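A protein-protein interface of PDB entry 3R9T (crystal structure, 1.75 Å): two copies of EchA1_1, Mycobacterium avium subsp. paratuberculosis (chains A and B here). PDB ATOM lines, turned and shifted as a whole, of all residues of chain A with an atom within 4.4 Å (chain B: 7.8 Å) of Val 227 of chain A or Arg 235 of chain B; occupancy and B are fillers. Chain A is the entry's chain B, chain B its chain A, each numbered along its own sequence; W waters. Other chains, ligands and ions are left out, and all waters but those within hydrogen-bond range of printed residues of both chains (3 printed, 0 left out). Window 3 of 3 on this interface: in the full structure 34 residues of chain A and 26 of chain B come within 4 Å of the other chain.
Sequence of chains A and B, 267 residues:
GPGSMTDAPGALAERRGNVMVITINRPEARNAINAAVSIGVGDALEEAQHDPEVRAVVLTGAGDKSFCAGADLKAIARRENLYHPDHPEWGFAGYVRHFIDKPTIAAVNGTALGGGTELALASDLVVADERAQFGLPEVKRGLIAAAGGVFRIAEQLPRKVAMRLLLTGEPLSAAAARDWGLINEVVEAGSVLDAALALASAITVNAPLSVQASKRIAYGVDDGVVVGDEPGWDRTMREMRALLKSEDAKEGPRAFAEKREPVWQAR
The side-chain carboxylate (OD1) of Asp 222 of chain A is in salt-bridge range of the guanidinium group (NE) of Arg 235 of chain B, at 2.9 Å. The guanidinium group of Arg 238 of chain B lies within hydrogen-bond range of the backbone carbonyl oxygen of Val 221 of chain A (2.9 Å). The guanidinium group of Arg 238 of chain B lies within salt-bridge range of the side-chain carboxylate of Asp 222 of chain A (2.8 Å).
The side-chain hydroxyl of Thr 236 of chain B is in hydrogen-bond range of the backbone carbonyl oxygen of Gly 232 of chain B, at 2.7 Å. The backbone NH of Val 227 of chain A is in hydrogen-bond range of the backbone carbonyl oxygen of Gly 220 of chain A (3.2 Å).
Ile 217 of chain A touches Ile 144 of chain B (CD1 to CD1, 3.5 Å). Ile 217 of chain A touches Thr 236 of chain B (CG2 to OG1, 3.6 Å). Glu 239 of chain B touches Ile 217 of chain A (CG to CD1, 3.8 Å). Arg 235 of chain B touches Gly 220 of chain A (NH1 to CA, 3.5 Å). Arg 235 of chain B touches Val 221 of chain A (NE to O, 3.9 Å). NH2 of Arg 235 of chain B touches CG2 of Val 227 of chain A (3.99 Å).
Printed residues of chain B within 4 Å of Val 221 of chain A: Arg 235 and Arg 238. Of the printed residues of chain B, Val 227 of chain A touches Arg 235. Printed residues of chain A within 4 Å of Thr 236 of chain B: Ile 217. The nearest printed residue of chain A that does not touch Arg 235 of chain B is Ile 217 of chain A (4.1 Å).
Of the 11 printed residues of chain A, 5 touch a printed residue of chain B. Printed residues of chain A that touch a printed residue of chain B: Ile 217, Gly 220, Val 221, Asp 222 and Val 227. Hydrophobic or aromatic side chains of chain A that line the printed part of chain B: Ile 217 and Val 227. Along chain A the printed residues that touch a printed residue of chain B span positions 217 to 227. Of the 16 printed residues of chain B, 5 touch a printed residue of chain A. Among the printed residues, Asp or Glu carboxylates within 4 Å of a Lys or Arg side-chain nitrogen of the other chain: Asp 222 of chain A with Arg 235 of chain B and Asp 222 of chain A with Arg 238 of chain B.
4 positions are printed for both chains.
Water W2 bridges the backbone carbonyl oxygen of Val 221 of chain A and the guanidinium group of Arg 238 of chain B. Water W1 lies within hydrogen-bond range of the guanidinium group (NH2) of Arg 238 of chain B (2.7 Å), the side-chain carboxylate (OE2) of Glu 239 of chain B (2.8 Å) and the backbone carbonyl oxygen (O) of Val 221 of chain A (3.3 Å). Water W3 bridges the backbone carbonyl oxygen of Ile 217 of chain A (2.8 Å) and the guanidinium group of Arg 235 of chain B (3.0 Å).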
ATOM      1  N   ILE A 217     -18.040 -21.167 -16.069  1.00  0.00           N
ATOM      2  CA  ILE A 217     -16.676 -21.366 -16.535  1.00  0.00           C
ATOM      3  C   ILE A 217     -16.462 -20.696 -17.893  1.00  0.00           C
ATOM      4  O   ILE A 217     -15.456 -20.039 -18.095  1.00  0.00           O
ATOM      5  CB  ILE A 217     -16.317 -22.845 -16.679  1.00  0.00           C
ATOM      6  CG1 ILE A 217     -16.322 -23.540 -15.333  1.00  0.00           C
ATOM      7  CG2 ILE A 217     -14.928 -22.997 -17.316  1.00  0.00           C
ATOM      8  CD1 ILE A 217     -16.622 -25.041 -15.403  1.00  0.00           C
ATOM      9  N   GLY A 220     -15.942 -17.079 -17.520  1.00  0.00           N
ATOM     10  CA  GLY A 220     -14.928 -16.633 -16.555  1.00  0.00           C
ATOM     11  C   GLY A 220     -15.509 -15.867 -15.391  1.00  0.00           C
ATOM     12  O   GLY A 220     -15.054 -14.786 -15.066  1.00  0.00           O
ATOM     13  N   VAL A 221     -16.498 -16.459 -14.735  1.00  0.00           N
ATOM     14  CA  VAL A 221     -17.226 -15.793 -13.672  1.00  0.00           C
ATOM     15  C   VAL A 221     -16.673 -16.157 -12.313  1.00  0.00           C
ATOM     16  O   VAL A 221     -16.584 -17.333 -11.959  1.00  0.00           O
ATOM     17  CB  VAL A 221     -18.718 -16.139 -13.744  1.00  0.00           C
ATOM     18  CG1 VAL A 221     -19.508 -15.573 -12.512  1.00  0.00           C
ATOM     19  CG2 VAL A 221     -19.271 -15.650 -15.101  1.00  0.00           C
ATOM     20  N   ASP A 222     -16.281 -15.118 -11.583  1.00  0.00           N
ATOM     21  CA  ASP A 222     -15.954 -15.212 -10.171  1.00  0.00           C
ATOM     22  C   ASP A 222     -16.956 -14.342  -9.401  1.00  0.00           C
ATOM     23  O   ASP A 222     -17.151 -13.167  -9.723  1.00  0.00           O
ATOM     24  CB  ASP A 222     -14.519 -14.733  -9.907  1.00  0.00           C
ATOM     25  CG  ASP A 222     -13.469 -15.566 -10.634  1.00  0.00           C
ATOM     26  OD1 ASP A 222     -13.676 -16.782 -10.844  1.00  0.00           O
ATOM     27  OD2 ASP A 222     -12.414 -14.993 -10.986  1.00  0.00           O
ATOM     28  N   VAL A 225     -19.504 -12.110 -11.304  1.00  0.00           N
ATOM     29  CA  VAL A 225     -18.957 -11.110 -12.229  1.00  0.00           C
ATOM     30  C   VAL A 225     -18.183 -11.768 -13.368  1.00  0.00           C
ATOM     31  O   VAL A 225     -17.356 -12.636 -13.126  1.00  0.00           O
ATOM     32  CB  VAL A 225     -17.995 -10.142 -11.497  1.00  0.00           C
ATOM     33  CG1 VAL A 225     -17.398  -9.119 -12.469  1.00  0.00           C
ATOM     34  CG2 VAL A 225     -18.731  -9.438 -10.372  1.00  0.00           C
ATOM     35  N   VAL A 226     -18.451 -11.336 -14.597  1.00  0.00           N
ATOM     36  CA  VAL A 226     -17.670 -11.739 -15.763  1.00  0.00           C
ATOM     37  C   VAL A 226     -16.372 -10.922 -15.704  1.00  0.00           C
ATOM     38  O   VAL A 226     -16.313  -9.767 -16.123  1.00  0.00           O
ATOM     39  CB  VAL A 226     -18.438 -11.508 -17.075  1.00  0.00           C
ATOM     40  CG1 VAL A 226     -17.602 -11.934 -18.301  1.00  0.00           C
ATOM     41  CG2 VAL A 226     -19.776 -12.266 -17.032  1.00  0.00           C
ATOM     42  N   VAL A 227     -15.325 -11.565 -15.200  1.00  0.00           N
ATOM     43  CA  VAL A 227     -14.058 -10.907 -14.882  1.00  0.00           C
ATOM     44  C   VAL A 227     -13.416 -10.228 -16.074  1.00  0.00           C
ATOM     45  O   VAL A 227     -12.906  -9.101 -15.972  1.00  0.00           O
ATOM     46  CB  VAL A 227     -13.059 -11.951 -14.346  1.00  0.00           C
ATOM     47  CG1 VAL A 227     -11.663 -11.361 -14.223  1.00  0.00           C
ATOM     48  CG2 VAL A 227     -13.545 -12.487 -13.027  1.00  0.00           C
ATOM     49  N   GLY A 228     -13.426 -10.930 -17.195  1.00  0.00           N
ATOM     50  CA  GLY A 228     -12.759 -10.462 -18.398  1.00  0.00           C
ATOM     51  C   GLY A 228     -13.369  -9.218 -19.022  1.00  0.00           C
ATOM     52  O   GLY A 228     -12.699  -8.530 -19.795  1.00  0.00           O
ATOM     53  N   ASP A 229     -14.631  -8.918 -18.693  1.00  0.00           N
ATOM     54  CA  ASP A 229     -15.297  -7.721 -19.224  1.00  0.00           C
ATOM     55  C   ASP A 229     -14.959  -6.422 -18.490  1.00  0.00           C
ATOM     56  O   ASP A 229     -15.249  -5.325 -18.994  1.00  0.00           O
ATOM     57  CB  ASP A 229     -16.817  -7.882 -19.186  1.00  0.00           C
ATOM     58  CG  ASP A 229     -17.345  -8.879 -20.186  1.00  0.00           C
ATOM     59  OD1 ASP A 229     -16.584  -9.338 -21.086  1.00  0.00           O
ATOM     60  OD2 ASP A 229     -18.560  -9.188 -20.054  1.00  0.00           O
ATOM     61  N   GLU A 230     -14.364  -6.529 -17.309  1.00  0.00           N
ATOM     62  CA  GLU A 230     -14.177  -5.354 -16.463  1.00  0.00           C
ATOM     63  C   GLU A 230     -13.326  -4.254 -17.121  1.00  0.00           C
ATOM     64  O   GLU A 230     -13.706  -3.084 -17.078  1.00  0.00           O
ATOM     65  CB  GLU A 230     -13.684  -5.758 -15.074  1.00  0.00           C
ATOM     66  CG  GLU A 230     -14.744  -6.594 -14.342  1.00  0.00           C
ATOM     67  CD  GLU A 230     -16.069  -5.844 -14.198  1.00  0.00           C
ATOM     68  OE1 GLU A 230     -17.108  -6.303 -14.726  1.00  0.00           O
ATOM     69  OE2 GLU A 230     -16.066  -4.764 -13.579  1.00  0.00           O
ATOM     70  N   PRO A 231     -12.230  -4.629 -17.801  1.00  0.00           N
ATOM     71  CA  PRO A 231     -11.464  -3.584 -18.483  1.00  0.00           C
ATOM     72  C   PRO A 231     -12.256  -2.916 -19.603  1.00  0.00           C
ATOM     73  O   PRO A 231     -12.153  -1.711 -19.775  1.00  0.00           O
ATOM     74  CB  PRO A 231     -10.239  -4.332 -19.024  1.00  0.00           C
ATOM     75  CG  PRO A 231     -10.104  -5.506 -18.103  1.00  0.00           C
ATOM     76  CD  PRO A 231     -11.514  -5.913 -17.805  1.00  0.00           C
ATOM     77  N   ILE B 144     -19.601 -32.104 -16.615  1.00  0.00           N
ATOM     78  CA  ILE B 144     -19.222 -30.983 -17.509  1.00  0.00           C
ATOM     79  C   ILE B 144     -17.989 -31.428 -18.296  1.00  0.00           C
ATOM     80  O   ILE B 144     -17.357 -32.425 -17.932  1.00  0.00           O
ATOM     81  CB  ILE B 144     -18.935 -29.635 -16.766  1.00  0.00           C
ATOM     82  CG1 ILE B 144     -17.873 -29.801 -15.673  1.00  0.00           C
ATOM     83  CG2 ILE B 144     -20.222 -29.043 -16.156  1.00  0.00           C
ATOM     84  CD1 ILE B 144     -17.290 -28.483 -15.129  1.00  0.00           C
ATOM     85  N   PHE B 151     -14.006 -24.135 -21.391  1.00  0.00           N
ATOM     86  CA  PHE B 151     -13.368 -22.855 -21.709  1.00  0.00           C
ATOM     87  C   PHE B 151     -12.687 -22.786 -23.068  1.00  0.00           C
ATOM     88  O   PHE B 151     -12.416 -21.678 -23.569  1.00  0.00           O
ATOM     89  CB  PHE B 151     -12.422 -22.390 -20.571  1.00  0.00           C
ATOM     90  CG  PHE B 151     -11.162 -23.216 -20.386  1.00  0.00           C
ATOM     91  CD1 PHE B 151     -11.116 -24.271 -19.477  1.00  0.00           C
ATOM     92  CD2 PHE B 151      -9.984 -22.863 -21.036  1.00  0.00           C
ATOM     93  CE1 PHE B 151      -9.940 -24.995 -19.291  1.00  0.00           C
ATOM     94  CE2 PHE B 151      -8.800 -23.591 -20.843  1.00  0.00           C
ATOM     95  CZ  PHE B 151      -8.787 -24.657 -19.971  1.00  0.00           C
ATOM     96  N   GLY B 228      -1.974 -18.627 -20.063  1.00  0.00           N
ATOM     97  CA  GLY B 228      -3.309 -18.082 -20.261  1.00  0.00           C
ATOM     98  C   GLY B 228      -4.453 -19.041 -19.952  1.00  0.00           C
ATOM     99  O   GLY B 228      -5.598 -18.610 -19.848  1.00  0.00           O
ATOM    100  N   ASP B 229      -4.167 -20.334 -19.821  1.00  0.00           N
ATOM    101  CA  ASP B 229      -5.223 -21.318 -19.575  1.00  0.00           C
ATOM    102  C   ASP B 229      -5.435 -21.534 -18.099  1.00  0.00           C
ATOM    103  O   ASP B 229      -6.381 -22.198 -17.712  1.00  0.00           O
ATOM    104  CB  ASP B 229      -4.863 -22.672 -20.188  1.00  0.00           C
ATOM    105  CG  ASP B 229      -5.055 -22.723 -21.688  1.00  0.00           C
ATOM    106  OD1 ASP B 229      -5.592 -21.756 -22.288  1.00  0.00           O
ATOM    107  OD2 ASP B 229      -4.666 -23.761 -22.267  1.00  0.00           O
ATOM    108  N   GLU B 230      -4.534 -21.018 -17.271  1.00  0.00           N
ATOM    109  CA  GLU B 230      -4.619 -21.252 -15.839  1.00  0.00           C
ATOM    110  C   GLU B 230      -5.978 -20.916 -15.221  1.00  0.00           C
ATOM    111  O   GLU B 230      -6.515 -21.756 -14.513  1.00  0.00           O
ATOM    112  CB  GLU B 230      -3.476 -20.557 -15.113  1.00  0.00           C
ATOM    113  CG  GLU B 230      -2.192 -21.301 -15.313  1.00  0.00           C
ATOM    114  CD  GLU B 230      -1.032 -20.631 -14.641  1.00  0.00           C
ATOM    115  OE1 GLU B 230      -1.189 -19.464 -14.207  1.00  0.00           O
ATOM    116  OE2 GLU B 230       0.035 -21.274 -14.538  1.00  0.00           O
ATOM    117  N   PRO B 231      -6.537 -19.711 -15.488  1.00  0.00           N
ATOM    118  CA  PRO B 231      -7.834 -19.395 -14.905  1.00  0.00           C
ATOM    119  C   PRO B 231      -8.918 -20.376 -15.331  1.00  0.00           C
ATOM    120  O   PRO B 231      -9.715 -20.787 -14.492  1.00  0.00           O
ATOM    121  CB  PRO B 231      -8.121 -17.984 -15.415  1.00  0.00           C
ATOM    122  CG  PRO B 231      -6.802 -17.424 -15.722  1.00  0.00           C
ATOM    123  CD  PRO B 231      -6.021 -18.571 -16.261  1.00  0.00           C
ATOM    124  N   GLY B 232      -8.935 -20.781 -16.598  1.00  0.00           N
ATOM    125  CA  GLY B 232      -9.928 -21.763 -17.054  1.00  0.00           C
ATOM    126  C   GLY B 232      -9.781 -23.112 -16.353  1.00  0.00           C
ATOM    127  O   GLY B 232     -10.766 -23.707 -15.916  1.00  0.00           O
ATOM    128  N   TRP B 233      -8.550 -23.592 -16.214  1.00  0.00           N
ATOM    129  CA  TRP B 233      -8.332 -24.846 -15.498  1.00  0.00           C
ATOM    130  C   TRP B 233      -8.779 -24.716 -14.037  1.00  0.00           C
ATOM    131  O   TRP B 233      -9.417 -25.616 -13.486  1.00  0.00           O
ATOM    132  CB  TRP B 233      -6.880 -25.305 -15.593  1.00  0.00           C
ATOM    133  CG  TRP B 233      -6.512 -25.846 -16.922  1.00  0.00           C
ATOM    134  CD1 TRP B 233      -5.513 -25.388 -17.734  1.00  0.00           C
ATOM    135  CD2 TRP B 233      -7.135 -26.935 -17.629  1.00  0.00           C
ATOM    136  NE1 TRP B 233      -5.453 -26.137 -18.882  1.00  0.00           N
ATOM    137  CE2 TRP B 233      -6.430 -27.095 -18.849  1.00  0.00           C
ATOM    138  CE3 TRP B 233      -8.178 -27.821 -17.332  1.00  0.00           C
ATOM    139  CZ2 TRP B 233      -6.757 -28.079 -19.792  1.00  0.00           C
ATOM    140  CZ3 TRP B 233      -8.515 -28.787 -18.281  1.00  0.00           C
ATOM    141  CH2 TRP B 233      -7.798 -28.914 -19.497  1.00  0.00           C
ATOM    142  N   ASP B 234      -8.439 -23.598 -13.412  1.00  0.00           N
ATOM    143  CA  ASP B 234      -8.763 -23.392 -12.009  1.00  0.00           C
ATOM    144  C   ASP B 234     -10.272 -23.326 -11.792  1.00  0.00           C
ATOM    145  O   ASP B 234     -10.764 -23.960 -10.858  1.00  0.00           O
ATOM    146  CB  ASP B 234      -8.050 -22.146 -11.464  1.00  0.00           C
ATOM    147  CG  ASP B 234      -6.530 -22.339 -11.349  1.00  0.00           C
ATOM    148  OD1 ASP B 234      -6.039 -23.494 -11.332  1.00  0.00           O
ATOM    149  OD2 ASP B 234      -5.830 -21.316 -11.267  1.00  0.00           O
ATOM    150  N   ARG B 235     -11.006 -22.607 -12.651  1.00  0.00           N
ATOM    151  CA  ARG B 235     -12.461 -22.552 -12.509  1.00  0.00           C
ATOM    152  C   ARG B 235     -13.068 -23.919 -12.809  1.00  0.00           C
ATOM    153  O   ARG B 235     -13.970 -24.367 -12.104  1.00  0.00           O
ATOM    154  CB  ARG B 235     -13.115 -21.506 -13.419  1.00  0.00           C
ATOM    155  CG  ARG B 235     -12.793 -20.091 -13.084  1.00  0.00           C
ATOM    156  CD  ARG B 235     -13.636 -19.058 -13.838  1.00  0.00           C
ATOM    157  NE  ARG B 235     -13.082 -17.755 -13.506  1.00  0.00           N
ATOM    158  CZ  ARG B 235     -12.159 -17.099 -14.212  1.00  0.00           C
ATOM    159  NH1 ARG B 235     -11.729 -17.541 -15.391  1.00  0.00           N
ATOM    160  NH2 ARG B 235     -11.686 -15.949 -13.744  1.00  0.00           N
ATOM    161  N   THR B 236     -12.558 -24.594 -13.834  1.00  0.00           N
ATOM    162  CA  THR B 236     -13.057 -25.917 -14.178  1.00  0.00           C
ATOM    163  C   THR B 236     -12.898 -26.892 -13.011  1.00  0.00           C
ATOM    164  O   THR B 236     -13.829 -27.620 -12.657  1.00  0.00           O
ATOM    165  CB  THR B 236     -12.345 -26.471 -15.383  1.00  0.00           C
ATOM    166  OG1 THR B 236     -12.635 -25.629 -16.515  1.00  0.00           O
ATOM    167  CG2 THR B 236     -12.825 -27.904 -15.682  1.00  0.00           C
ATOM    168  N   MET B 237     -11.713 -26.892 -12.430  1.00  0.00           N
ATOM    169  CA  MET B 237     -11.390 -27.804 -11.341  1.00  0.00           C
ATOM    170  C   MET B 237     -12.271 -27.533 -10.118  1.00  0.00           C
ATOM    171  O   MET B 237     -12.810 -28.466  -9.532  1.00  0.00           O
ATOM    172  CB  MET B 237      -9.900 -27.686 -11.015  1.00  0.00           C
ATOM    173  CG  MET B 237      -9.024 -28.359 -12.056  1.00  0.00           C
ATOM    174  SD  MET B 237      -7.235 -28.127 -11.820  1.00  0.00           S
ATOM    175  CE  MET B 237      -6.958 -29.130 -10.353  1.00  0.00           C
ATOM    176  N   ARG B 238     -12.469 -26.265  -9.773  1.00  0.00           N
ATOM    177  CA  ARG B 238     -13.261 -25.920  -8.586  1.00  0.00           C
ATOM    178  C   ARG B 238     -14.735 -26.299  -8.804  1.00  0.00           C
ATOM    179  O   ARG B 238     -15.379 -26.852  -7.913  1.00  0.00           O
ATOM    180  CB  ARG B 238     -13.052 -24.446  -8.185  1.00  0.00           C
ATOM    181  CG  ARG B 238     -14.179 -23.463  -8.508  1.00  0.00           C
ATOM    182  CD  ARG B 238     -13.786 -21.989  -8.242  1.00  0.00           C
ATOM    183  NE  ARG B 238     -14.557 -21.105  -9.125  1.00  0.00           N
ATOM    184  CZ  ARG B 238     -14.182 -19.899  -9.568  1.00  0.00           C
ATOM    185  NH1 ARG B 238     -13.021 -19.340  -9.224  1.00  0.00           N
ATOM    186  NH2 ARG B 238     -14.992 -19.236 -10.378  1.00  0.00           N
ATOM    187  N   GLU B 239     -15.241 -26.059 -10.008  1.00  0.00           N
ATOM    188  CA  GLU B 239     -16.610 -26.474 -10.360  1.00  0.00           C
ATOM    189  C   GLU B 239     -16.820 -27.999 -10.403  1.00  0.00           C
ATOM    190  O   GLU B 239     -17.847 -28.497  -9.939  1.00  0.00           O
ATOM    191  CB  GLU B 239     -17.016 -25.870 -11.704  1.00  0.00           C
ATOM    192  CG  GLU B 239     -17.083 -24.354 -11.713  1.00  0.00           C
ATOM    193  CD  GLU B 239     -18.354 -23.765 -11.131  1.00  0.00           C
ATOM    194  OE1 GLU B 239     -19.242 -24.523 -10.655  1.00  0.00           O
ATOM    195  OE2 GLU B 239     -18.450 -22.510 -11.172  1.00  0.00           O
ATOM    196  N   MET B 240     -15.867 -28.732 -10.979  1.00  0.00           N
ATOM    197  CA  MET B 240     -16.001 -30.170 -11.148  1.00  0.00           C
ATOM    198  C   MET B 240     -16.046 -30.836  -9.781  1.00  0.00           C
ATOM    199  O   MET B 240     -16.899 -31.686  -9.522  1.00  0.00           O
ATOM    200  CB  MET B 240     -14.836 -30.729 -11.982  1.00  0.00           C
ATOM    201  CG  MET B 240     -14.999 -32.186 -12.419  1.00  0.00           C
ATOM    202  SD  MET B 240     -16.516 -32.489 -13.324  1.00  0.00           S
ATOM    203  CE  MET B 240     -16.130 -34.085 -14.072  1.00  0.00           C
ATOM    204  N   ARG B 241     -15.152 -30.415  -8.893  1.00  0.00           N
ATOM    205  CA  ARG B 241     -15.121 -30.973  -7.542  1.00  0.00           C
ATOM    206  C   ARG B 241     -16.457 -30.802  -6.824  1.00  0.00           C
ATOM    207  O   ARG B 241     -16.918 -31.728  -6.152  1.00  0.00           O
ATOM    208  CB  ARG B 241     -13.979 -30.374  -6.724  1.00  0.00           C
ATOM    209  CG  ARG B 241     -12.595 -30.757  -7.245  1.00  0.00           C
ATOM    210  CD  ARG B 241     -11.523 -30.532  -6.201  1.00  0.00           C
ATOM    211  NE  ARG B 241     -11.708 -31.478  -5.102  1.00  0.00           N
ATOM    212  CZ  ARG B 241     -11.076 -32.643  -4.973  1.00  0.00           C
ATOM    213  NH1 ARG B 241     -10.151 -33.028  -5.849  1.00  0.00           N
ATOM    214  NH2 ARG B 241     -11.359 -33.421  -3.936  1.00  0.00           N
HETATM  215  O   HOH W   1     -16.554 -20.655 -12.141  1.00  0.00           O
HETATM  216  O   HOH W   2     -18.190 -18.523 -10.117  1.00  0.00           O
HETATM  217  O   HOH W   3     -12.890 -19.693 -17.133  1.00  0.00           O
